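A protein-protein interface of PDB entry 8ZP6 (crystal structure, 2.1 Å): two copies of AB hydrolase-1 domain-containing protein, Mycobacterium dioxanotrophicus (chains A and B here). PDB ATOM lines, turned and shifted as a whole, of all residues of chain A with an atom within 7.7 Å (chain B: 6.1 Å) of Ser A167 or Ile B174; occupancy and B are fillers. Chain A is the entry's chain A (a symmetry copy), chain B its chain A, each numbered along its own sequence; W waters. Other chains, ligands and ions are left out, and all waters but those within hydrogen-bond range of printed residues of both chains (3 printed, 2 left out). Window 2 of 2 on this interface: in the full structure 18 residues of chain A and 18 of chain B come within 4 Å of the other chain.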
ATOM      1  N   ASP A 159     -31.710 -22.313  22.028  1.00  0.00           N
ATOM      2  CA  ASP A 159     -30.517 -21.659  21.502  1.00  0.00           C
ATOM      3  C   ASP A 159     -29.435 -22.689  21.209  1.00  0.00           C
ATOM      4  O   ASP A 159     -28.653 -22.536  20.269  1.00  0.00           O
ATOM      5  CB  ASP A 159     -29.996 -20.603  22.474  1.00  0.00           C
ATOM      6  CG  ASP A 159     -30.873 -19.368  22.505  1.00  0.00           C
ATOM      7  OD1 ASP A 159     -31.504 -19.057  21.471  1.00  0.00           O
ATOM      8  OD2 ASP A 159     -30.947 -18.723  23.563  1.00  0.00           O
ATOM      9  N   MET A 160     -29.394 -23.743  22.015  1.00  0.00           N
ATOM     10  CA  MET A 160     -28.353 -24.746  21.868  1.00  0.00           C
ATOM     11  C   MET A 160     -28.424 -25.434  20.509  1.00  0.00           C
ATOM     12  O   MET A 160     -27.395 -25.799  19.959  1.00  0.00           O
ATOM     13  CB  MET A 160     -28.428 -25.785  22.993  1.00  0.00           C
ATOM     14  CG  MET A 160     -27.359 -26.876  22.883  1.00  0.00           C
ATOM     15  SD  MET A 160     -27.898 -28.304  21.909  1.00  0.00           S
ATOM     16  CE  MET A 160     -28.934 -29.123  23.136  1.00  0.00           C
ATOM     17  N   SER A 161     -29.624 -25.607  19.958  1.00  0.00           N
ATOM     18  CA  SER A 161     -29.730 -26.236  18.650  1.00  0.00           C
ATOM     19  C   SER A 161     -28.955 -25.448  17.591  1.00  0.00           C
ATOM     20  O   SER A 161     -28.239 -26.040  16.801  1.00  0.00           O
ATOM     21  CB  SER A 161     -31.192 -26.400  18.221  1.00  0.00           C
ATOM     22  OG  SER A 161     -31.849 -25.156  18.127  1.00  0.00           O
ATOM     23  N   VAL A 162     -29.085 -24.126  17.579  1.00  0.00           N
ATOM     24  CA  VAL A 162     -28.335 -23.317  16.615  1.00  0.00           C
ATOM     25  C   VAL A 162     -26.829 -23.439  16.862  1.00  0.00           C
ATOM     26  O   VAL A 162     -26.056 -23.657  15.935  1.00  0.00           O
ATOM     27  CB  VAL A 162     -28.735 -21.815  16.667  1.00  0.00           C
ATOM     28  CG1 VAL A 162     -27.896 -20.992  15.675  1.00  0.00           C
ATOM     29  CG2 VAL A 162     -30.222 -21.631  16.389  1.00  0.00           C
ATOM     30  N   GLU A 163     -26.427 -23.313  18.122  1.00  0.00           N
ATOM     31  CA  GLU A 163     -25.016 -23.385  18.493  1.00  0.00           C
ATOM     32  C   GLU A 163     -24.404 -24.705  18.055  1.00  0.00           C
ATOM     33  O   GLU A 163     -23.306 -24.741  17.493  1.00  0.00           O
ATOM     34  CB  GLU A 163     -24.850 -23.203  20.009  1.00  0.00           C
ATOM     35  CG  GLU A 163     -23.399 -23.148  20.459  1.00  0.00           C
ATOM     36  CD  GLU A 163     -23.234 -23.090  21.975  1.00  0.00           C
ATOM     37  OE1 GLU A 163     -24.220 -23.298  22.723  1.00  0.00           O
ATOM     38  OE2 GLU A 163     -22.101 -22.816  22.415  1.00  0.00           O
ATOM     39  N   LEU A 164     -25.132 -25.793  18.292  1.00  0.00           N
ATOM     40  CA  LEU A 164     -24.640 -27.130  17.966  1.00  0.00           C
ATOM     41  C   LEU A 164     -24.558 -27.363  16.456  1.00  0.00           C
ATOM     42  O   LEU A 164     -23.535 -27.804  15.937  1.00  0.00           O
ATOM     43  CB  LEU A 164     -25.536 -28.200  18.604  1.00  0.00           C
ATOM     44  CG  LEU A 164     -25.177 -29.663  18.304  1.00  0.00           C
ATOM     45  CD1 LEU A 164     -23.732 -29.945  18.716  1.00  0.00           C
ATOM     46  CD2 LEU A 164     -26.110 -30.616  19.022  1.00  0.00           C
ATOM     47  N   VAL A 165     -25.652 -27.086  15.759  1.00  0.00           N
ATOM     48  CA  VAL A 165     -25.741 -27.399  14.338  1.00  0.00           C
ATOM     49  C   VAL A 165     -24.788 -26.526  13.498  1.00  0.00           C
ATOM     50  O   VAL A 165     -24.284 -26.975  12.477  1.00  0.00           O
ATOM     51  CB  VAL A 165     -27.211 -27.269  13.851  1.00  0.00           C
ATOM     52  CG1 VAL A 165     -27.326 -27.438  12.344  1.00  0.00           C
ATOM     53  CG2 VAL A 165     -28.068 -28.337  14.542  1.00  0.00           C
ATOM     54  N   THR A 166     -24.502 -25.306  13.946  1.00  0.00           N
ATOM     55  CA  THR A 166     -23.580 -24.432  13.208  1.00  0.00           C
ATOM     56  C   THR A 166     -22.151 -24.483  13.745  1.00  0.00           C
ATOM     57  O   THR A 166     -21.304 -23.721  13.292  1.00  0.00           O
ATOM     58  CB  THR A 166     -24.028 -22.961  13.241  1.00  0.00           C
ATOM     59  OG1 THR A 166     -23.952 -22.461  14.586  1.00  0.00           O
ATOM     60  CG2 THR A 166     -25.445 -22.819  12.719  1.00  0.00           C
ATOM     61  N   SER A 167     -21.882 -25.365  14.707  1.00  0.00           N
ATOM     62  CA  SER A 167     -20.575 -25.383  15.371  1.00  0.00           C
ATOM     63  C   SER A 167     -19.463 -25.771  14.401  1.00  0.00           C
ATOM     64  O   SER A 167     -18.314 -25.385  14.578  1.00  0.00           O
ATOM     65  CB  SER A 167     -20.578 -26.324  16.588  1.00  0.00           C
ATOM     66  OG  SER A 167     -20.784 -27.685  16.240  1.00  0.00           O
ATOM     67  N   SER A 168     -19.813 -26.537  13.377  1.00  0.00           N
ATOM     68  CA  SER A 168     -18.873 -26.861  12.318  1.00  0.00           C
ATOM     69  C   SER A 168     -19.644 -27.372  11.121  1.00  0.00           C
ATOM     70  O   SER A 168     -20.805 -27.750  11.245  1.00  0.00           O
ATOM     71  CB  SER A 168     -17.844 -27.897  12.777  1.00  0.00           C
ATOM     72  OG  SER A 168     -18.426 -29.175  12.924  1.00  0.00           O
ATOM     73  N   ARG A 169     -19.002 -27.358   9.960  1.00  0.00           N
ATOM     74  CA  ARG A 169     -19.611 -27.863   8.748  1.00  0.00           C
ATOM     75  C   ARG A 169     -19.916 -29.350   8.915  1.00  0.00           C
ATOM     76  O   ARG A 169     -20.943 -29.840   8.457  1.00  0.00           O
ATOM     77  CB  ARG A 169     -18.688 -27.619   7.555  1.00  0.00           C
ATOM     78  CG  ARG A 169     -19.197 -28.208   6.279  1.00  0.00           C
ATOM     79  CD  ARG A 169     -18.281 -27.940   5.085  1.00  0.00           C
ATOM     80  NE  ARG A 169     -18.858 -28.582   3.914  1.00  0.00           N
ATOM     81  CZ  ARG A 169     -19.672 -27.977   3.055  1.00  0.00           C
ATOM     82  NH1 ARG A 169     -19.979 -26.685   3.205  1.00  0.00           N
ATOM     83  NH2 ARG A 169     -20.163 -28.660   2.029  1.00  0.00           N
ATOM     84  N   GLU A 170     -19.021 -30.056   9.595  1.00  0.00           N
ATOM     85  CA  GLU A 170     -19.217 -31.468   9.906  1.00  0.00           C
ATOM     86  C   GLU A 170     -20.465 -31.706  10.777  1.00  0.00           C
ATOM     87  O   GLU A 170     -21.255 -32.593  10.485  1.00  0.00           O
ATOM     88  CB  GLU A 170     -17.969 -32.026  10.599  1.00  0.00           C
ATOM     89  CG  GLU A 170     -18.124 -33.408  11.202  1.00  0.00           C
ATOM     90  CD  GLU A 170     -16.994 -33.766  12.179  1.00  0.00           C
ATOM     91  OE1 GLU A 170     -16.509 -32.872  12.926  1.00  0.00           O
ATOM     92  OE2 GLU A 170     -16.600 -34.952  12.200  1.00  0.00           O
ATOM     93  N   ALA A 171     -20.640 -30.931  11.843  1.00  0.00           N
ATOM     94  CA  ALA A 171     -21.836 -31.074  12.682  1.00  0.00           C
ATOM     95  C   ALA A 171     -23.104 -30.801  11.860  1.00  0.00           C
ATOM     96  O   ALA A 171     -24.097 -31.517  11.954  1.00  0.00           O
ATOM     97  CB  ALA A 171     -21.764 -30.130  13.885  1.00  0.00           C
ATOM     98  N   CYS A 172     -23.035 -29.759  11.040  1.00  0.00           N
ATOM     99  CA  CYS A 172     -24.136 -29.355  10.183  1.00  0.00           C
ATOM    100  C   CYS A 172     -24.544 -30.473   9.226  1.00  0.00           C
ATOM    101  O   CYS A 172     -25.725 -30.802   9.105  1.00  0.00           O
ATOM    102  CB  CYS A 172     -23.742 -28.094   9.401  1.00  0.00           C
ATOM    103  SG  CYS A 172     -25.095 -27.340   8.487  1.00  0.00           S
ATOM    104  N   MET A 203     -24.970 -23.446   5.921  1.00  0.00           N
ATOM    105  CA  MET A 203     -23.845 -22.824   6.606  1.00  0.00           C
ATOM    106  C   MET A 203     -23.684 -21.329   6.271  1.00  0.00           C
ATOM    107  O   MET A 203     -22.887 -20.639   6.904  1.00  0.00           O
ATOM    108  CB  MET A 203     -22.549 -23.577   6.283  1.00  0.00           C
ATOM    109  CG  MET A 203     -22.394 -24.927   6.996  1.00  0.00           C
ATOM    110  SD  MET A 203     -22.459 -24.829   8.796  1.00  0.00           S
ATOM    111  CE  MET A 203     -20.858 -24.100   9.138  1.00  0.00           C
ATOM    112  N   SER B 168     -17.350 -34.544  18.165  1.00  0.00           N
ATOM    113  CA  SER B 168     -16.184 -33.877  18.716  1.00  0.00           C
ATOM    114  C   SER B 168     -16.457 -33.536  20.165  1.00  0.00           C
ATOM    115  O   SER B 168     -17.604 -33.535  20.598  1.00  0.00           O
ATOM    116  CB  SER B 168     -15.832 -32.615  17.925  1.00  0.00           C
ATOM    117  OG  SER B 168     -16.773 -31.586  18.145  1.00  0.00           O
ATOM    118  N   ARG B 169     -15.394 -33.271  20.915  1.00  0.00           N
ATOM    119  CA  ARG B 169     -15.520 -32.887  22.304  1.00  0.00           C
ATOM    120  C   ARG B 169     -16.300 -31.577  22.399  1.00  0.00           C
ATOM    121  O   ARG B 169     -17.110 -31.386  23.300  1.00  0.00           O
ATOM    122  CB  ARG B 169     -14.138 -32.754  22.941  1.00  0.00           C
ATOM    123  CG  ARG B 169     -14.177 -32.254  24.350  1.00  0.00           C
ATOM    124  CD  ARG B 169     -12.793 -32.146  24.988  1.00  0.00           C
ATOM    125  NE  ARG B 169     -12.953 -31.625  26.338  1.00  0.00           N
ATOM    126  CZ  ARG B 169     -13.076 -32.383  27.422  1.00  0.00           C
ATOM    127  NH1 ARG B 169     -13.012 -33.714  27.331  1.00  0.00           N
ATOM    128  NH2 ARG B 169     -13.240 -31.807  28.606  1.00  0.00           N
ATOM    129  N   GLU B 170     -16.060 -30.685  21.445  1.00  0.00           N
ATOM    130  CA  GLU B 170     -16.789 -29.424  21.357  1.00  0.00           C
ATOM    131  C   GLU B 170     -18.300 -29.637  21.152  1.00  0.00           C
ATOM    132  O   GLU B 170     -19.104 -29.010  21.829  1.00  0.00           O
ATOM    133  CB  GLU B 170     -16.213 -28.568  20.225  1.00  0.00           C
ATOM    134  CG  GLU B 170     -17.027 -27.344  19.855  1.00  0.00           C
ATOM    135  CD  GLU B 170     -16.617 -26.735  18.506  1.00  0.00           C
ATOM    136  OE1 GLU B 170     -16.271 -27.493  17.559  1.00  0.00           O
ATOM    137  OE2 GLU B 170     -16.652 -25.490  18.399  1.00  0.00           O
ATOM    138  N   ALA B 171     -18.688 -30.504  20.221  1.00  0.00           N
ATOM    139  CA  ALA B 171     -20.114 -30.789  20.015  1.00  0.00           C
ATOM    140  C   ALA B 171     -20.736 -31.371  21.292  1.00  0.00           C
ATOM    141  O   ALA B 171     -21.831 -30.996  21.702  1.00  0.00           O
ATOM    142  CB  ALA B 171     -20.305 -31.753  18.840  1.00  0.00           C
ATOM    143  N   CYS B 172     -19.999 -32.281  21.917  1.00  0.00           N
ATOM    144  CA  CYS B 172     -20.425 -32.935  23.144  1.00  0.00           C
ATOM    145  C   CYS B 172     -20.680 -31.925  24.261  1.00  0.00           C
ATOM    146  O   CYS B 172     -21.722 -31.959  24.918  1.00  0.00           O
ATOM    147  CB  CYS B 172     -19.365 -33.958  23.575  1.00  0.00           C
ATOM    148  SG  CYS B 172     -19.873 -35.016  24.938  1.00  0.00           S
ATOM    149  N   ARG B 173     -19.727 -31.019  24.461  1.00  0.00           N
ATOM    150  CA  ARG B 173     -19.847 -29.978  25.474  1.00  0.00           C
ATOM    151  C   ARG B 173     -21.069 -29.090  25.231  1.00  0.00           C
ATOM    152  O   ARG B 173     -21.833 -28.813  26.146  1.00  0.00           O
ATOM    153  CB  ARG B 173     -18.579 -29.120  25.510  1.00  0.00           C
ATOM    154  CG  ARG B 173     -18.403 -28.316  26.793  1.00  0.00           C
ATOM    155  CD  ARG B 173     -17.399 -27.169  26.621  1.00  0.00           C
ATOM    156  NE  ARG B 173     -18.110 -25.947  26.249  1.00  0.00           N
ATOM    157  CZ  ARG B 173     -18.336 -25.545  24.999  1.00  0.00           C
ATOM    158  NH1 ARG B 173     -19.015 -24.428  24.781  1.00  0.00           N
ATOM    159  NH2 ARG B 173     -17.881 -26.249  23.967  1.00  0.00           N
ATOM    160  N   ILE B 174     -21.235 -28.646  23.990  1.00  0.00           N
ATOM    161  CA  ILE B 174     -22.362 -27.808  23.609  1.00  0.00           C
ATOM    162  C   ILE B 174     -23.694 -28.467  23.964  1.00  0.00           C
ATOM    163  O   ILE B 174     -24.572 -27.843  24.561  1.00  0.00           O
ATOM    164  CB  ILE B 174     -22.316 -27.495  22.097  1.00  0.00           C
ATOM    165  CG1 ILE B 174     -21.159 -26.521  21.802  1.00  0.00           C
ATOM    166  CG2 ILE B 174     -23.660 -26.926  21.608  1.00  0.00           C
ATOM    167  CD1 ILE B 174     -20.864 -26.341  20.334  1.00  0.00           C
ATOM    168  N   TYR B 175     -23.819 -29.741  23.616  1.00  0.00           N
ATOM    169  CA  TYR B 175     -25.060 -30.467  23.822  1.00  0.00           C
ATOM    170  C   TYR B 175     -25.397 -30.588  25.301  1.00  0.00           C
ATOM    171  O   TYR B 175     -26.457 -30.162  25.735  1.00  0.00           O
ATOM    172  CB  TYR B 175     -24.979 -31.853  23.184  1.00  0.00           C
ATOM    173  CG  TYR B 175     -26.285 -32.600  23.261  1.00  0.00           C
ATOM    174  CD1 TYR B 175     -27.353 -32.236  22.450  1.00  0.00           C
ATOM    175  CD2 TYR B 175     -26.457 -33.665  24.146  1.00  0.00           C
ATOM    176  CE1 TYR B 175     -28.554 -32.906  22.511  1.00  0.00           C
ATOM    177  CE2 TYR B 175     -27.658 -34.348  24.219  1.00  0.00           C
ATOM    178  CZ  TYR B 175     -28.704 -33.962  23.392  1.00  0.00           C
ATOM    179  OH  TYR B 175     -29.902 -34.618  23.441  1.00  0.00           O
ATOM    180  N   PHE B 176     -24.478 -31.154  26.079  1.00  0.00           N
ATOM    181  CA  PHE B 176     -24.763 -31.466  27.478  1.00  0.00           C
ATOM    182  C   PHE B 176     -24.889 -30.227  28.354  1.00  0.00           C
ATOM    183  O   PHE B 176     -25.652 -30.235  29.309  1.00  0.00           O
ATOM    184  CB  PHE B 176     -23.700 -32.427  28.033  1.00  0.00           C
ATOM    185  CG  PHE B 176     -23.846 -33.832  27.508  1.00  0.00           C
ATOM    186  CD1 PHE B 176     -24.894 -34.631  27.933  1.00  0.00           C
ATOM    187  CD2 PHE B 176     -22.974 -34.333  26.550  1.00  0.00           C
ATOM    188  CE1 PHE B 176     -25.057 -35.910  27.440  1.00  0.00           C
ATOM    189  CE2 PHE B 176     -23.131 -35.608  26.056  1.00  0.00           C
ATOM    190  CZ  PHE B 176     -24.172 -36.400  26.504  1.00  0.00           C
ATOM    191  N   LYS B 177     -24.169 -29.160  28.019  1.00  0.00           N
ATOM    192  CA  LYS B 177     -24.268 -27.918  28.784  1.00  0.00           C
ATOM    193  C   LYS B 177     -25.705 -27.390  28.855  1.00  0.00           C
ATOM    194  O   LYS B 177     -26.130 -26.869  29.882  1.00  0.00           O
ATOM    195  CB  LYS B 177     -23.363 -26.837  28.193  1.00  0.00           C
ATOM    196  CG  LYS B 177     -23.352 -25.558  29.008  1.00  0.00           C
ATOM    197  CD  LYS B 177     -22.143 -24.697  28.689  1.00  0.00           C
ATOM    198  CE  LYS B 177     -22.523 -23.499  27.848  1.00  0.00           C
ATOM    199  NZ  LYS B 177     -21.321 -22.835  27.255  1.00  0.00           N
ATOM    200  N   HIS B 178     -26.446 -27.532  27.761  1.00  0.00           N
ATOM    201  CA  HIS B 178     -27.836 -27.089  27.718  1.00  0.00           C
ATOM    202  C   HIS B 178     -28.654 -27.717  28.843  1.00  0.00           C
ATOM    203  O   HIS B 178     -29.424 -27.040  29.519  1.00  0.00           O
ATOM    204  CB  HIS B 178     -28.465 -27.432  26.364  1.00  0.00           C
ATOM    205  CG  HIS B 178     -29.959 -27.413  26.379  1.00  0.00           C
ATOM    206  ND1 HIS B 178     -30.685 -26.247  26.304  1.00  0.00           N
ATOM    207  CD2 HIS B 178     -30.864 -28.416  26.482  1.00  0.00           C
ATOM    208  CE1 HIS B 178     -31.975 -26.531  26.353  1.00  0.00           C
ATOM    209  NE2 HIS B 178     -32.111 -27.839  26.463  1.00  0.00           N
ATOM    210  N   PHE B 179     -28.472 -29.011  29.059  1.00  0.00           N
ATOM    211  CA  PHE B 179     -29.288 -29.710  30.046  1.00  0.00           C
ATOM    212  C   PHE B 179     -28.893 -29.357  31.473  1.00  0.00           C
ATOM    213  O   PHE B 179     -29.767 -29.130  32.303  1.00  0.00           O
ATOM    214  CB  PHE B 179     -29.218 -31.214  29.801  1.00  0.00           C
ATOM    215  CG  PHE B 179     -29.773 -31.608  28.463  1.00  0.00           C
ATOM    216  CD1 PHE B 179     -31.137 -31.790  28.295  1.00  0.00           C
ATOM    217  CD2 PHE B 179     -28.942 -31.737  27.368  1.00  0.00           C
ATOM    218  CE1 PHE B 179     -31.657 -32.126  27.057  1.00  0.00           C
ATOM    219  CE2 PHE B 179     -29.449 -32.059  26.120  1.00  0.00           C
ATOM    220  CZ  PHE B 179     -30.803 -32.262  25.958  1.00  0.00           C
HETATM  221  O   HOH W   1     -21.901 -23.772  24.930  1.00  0.00           O
HETATM  222  O   HOH W   2     -30.168 -23.578  25.064  1.00  0.00           O
HETATM  223  O   HOH W   3     -24.625 -25.276  25.026  1.00  0.00           O
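Water W1 lies within hydrogen-bond range of NZ of Lys B177 (2.6 Å), OE2 of Glu A163 (2.7 Å) and NH1 of Arg B173 (3.0 Å).
Water W3 bridges O of Ile B174 (2.6 Å) and OE1 of Glu A163 (3.1 Å).
Water W2 lies within hydrogen-bond range of ND1 of His B178 (3.0 Å) and N of Met A160 (3.2 Å).
O of Leu A164 is in hydrogen-bond range of OG of Ser A167, at 2.8 Å.
The side-chain hydroxyl (OG) of Ser B168 is in hydrogen-bond range of the backbone NH (N) of Ala B171 (3.0 Å).
Positions printed for both chains: 168, 169, 170, 171 and 172.
Of the 8 pairs that touch across the chains among the printed residues, none has its exchanged pair printed and touching as well.
Met A160 touches Ile B174 (CG to O, 3.4 Å).
Tyr B175 touches Met A160.
CB of His B178 touches CE of Met A160, 3.7 Å away.
Glu A163 touches Ile B174 (OE1 to CG2, 3.8 Å).
CD1 of Leu A164 touches O of Ala B171, at 3.7 Å.
Leu A164 touches Ile B174 (CB to CG2, 3.8 Å).
Leu A164 touches Tyr B175 (CD2 to CD1, 3.99 Å).
Ser A167 touches Ile B174.
Of the printed residues of chain B, Glu A163 touches Ile B174.
Of the printed residues of chain B, Leu A164 touches Ala B171 (3.7 Å), Ile B174 (3.8 Å) and Tyr B175 (3.99 Å).
Of chain B, only Ile B174 (3.8 Å) comes within 4 Å of Ser A167.
Of the printed residues of chain A, Ala B171 touches Leu A164 (3.7 Å).
Of chain A, only Met A160 (3.4 Å), Glu A163 (3.8 Å), Leu A164 (3.8 Å) and Ser A167 (3.8 Å) come within 4 Å of Ile B174.
Printed residues of chain A within 4 Å of Tyr B175: Met A160 (3.6 Å) and Leu A164 (3.99 Å).
Printed residues of chain A within 4 Å of His B178: Met A160 (3.7 Å).
The nearest residue of chain B that does not touch Ser A167 is Glu B170 (4.2 Å).
The nearest residue of chain A that does not touch Ile B174 is Val A165 (6.2 Å).
Hydrophobic or aromatic side chains of chain A that line the printed part of chain B: Met A160 and Leu A164.
Hydrophobic or aromatic side chains of chain B within 4 Å of the printed part of chain A: Ala B171, Ile B174, Tyr B175 and His B178.
Among the printed residues, 8 pairs touch across the chains.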
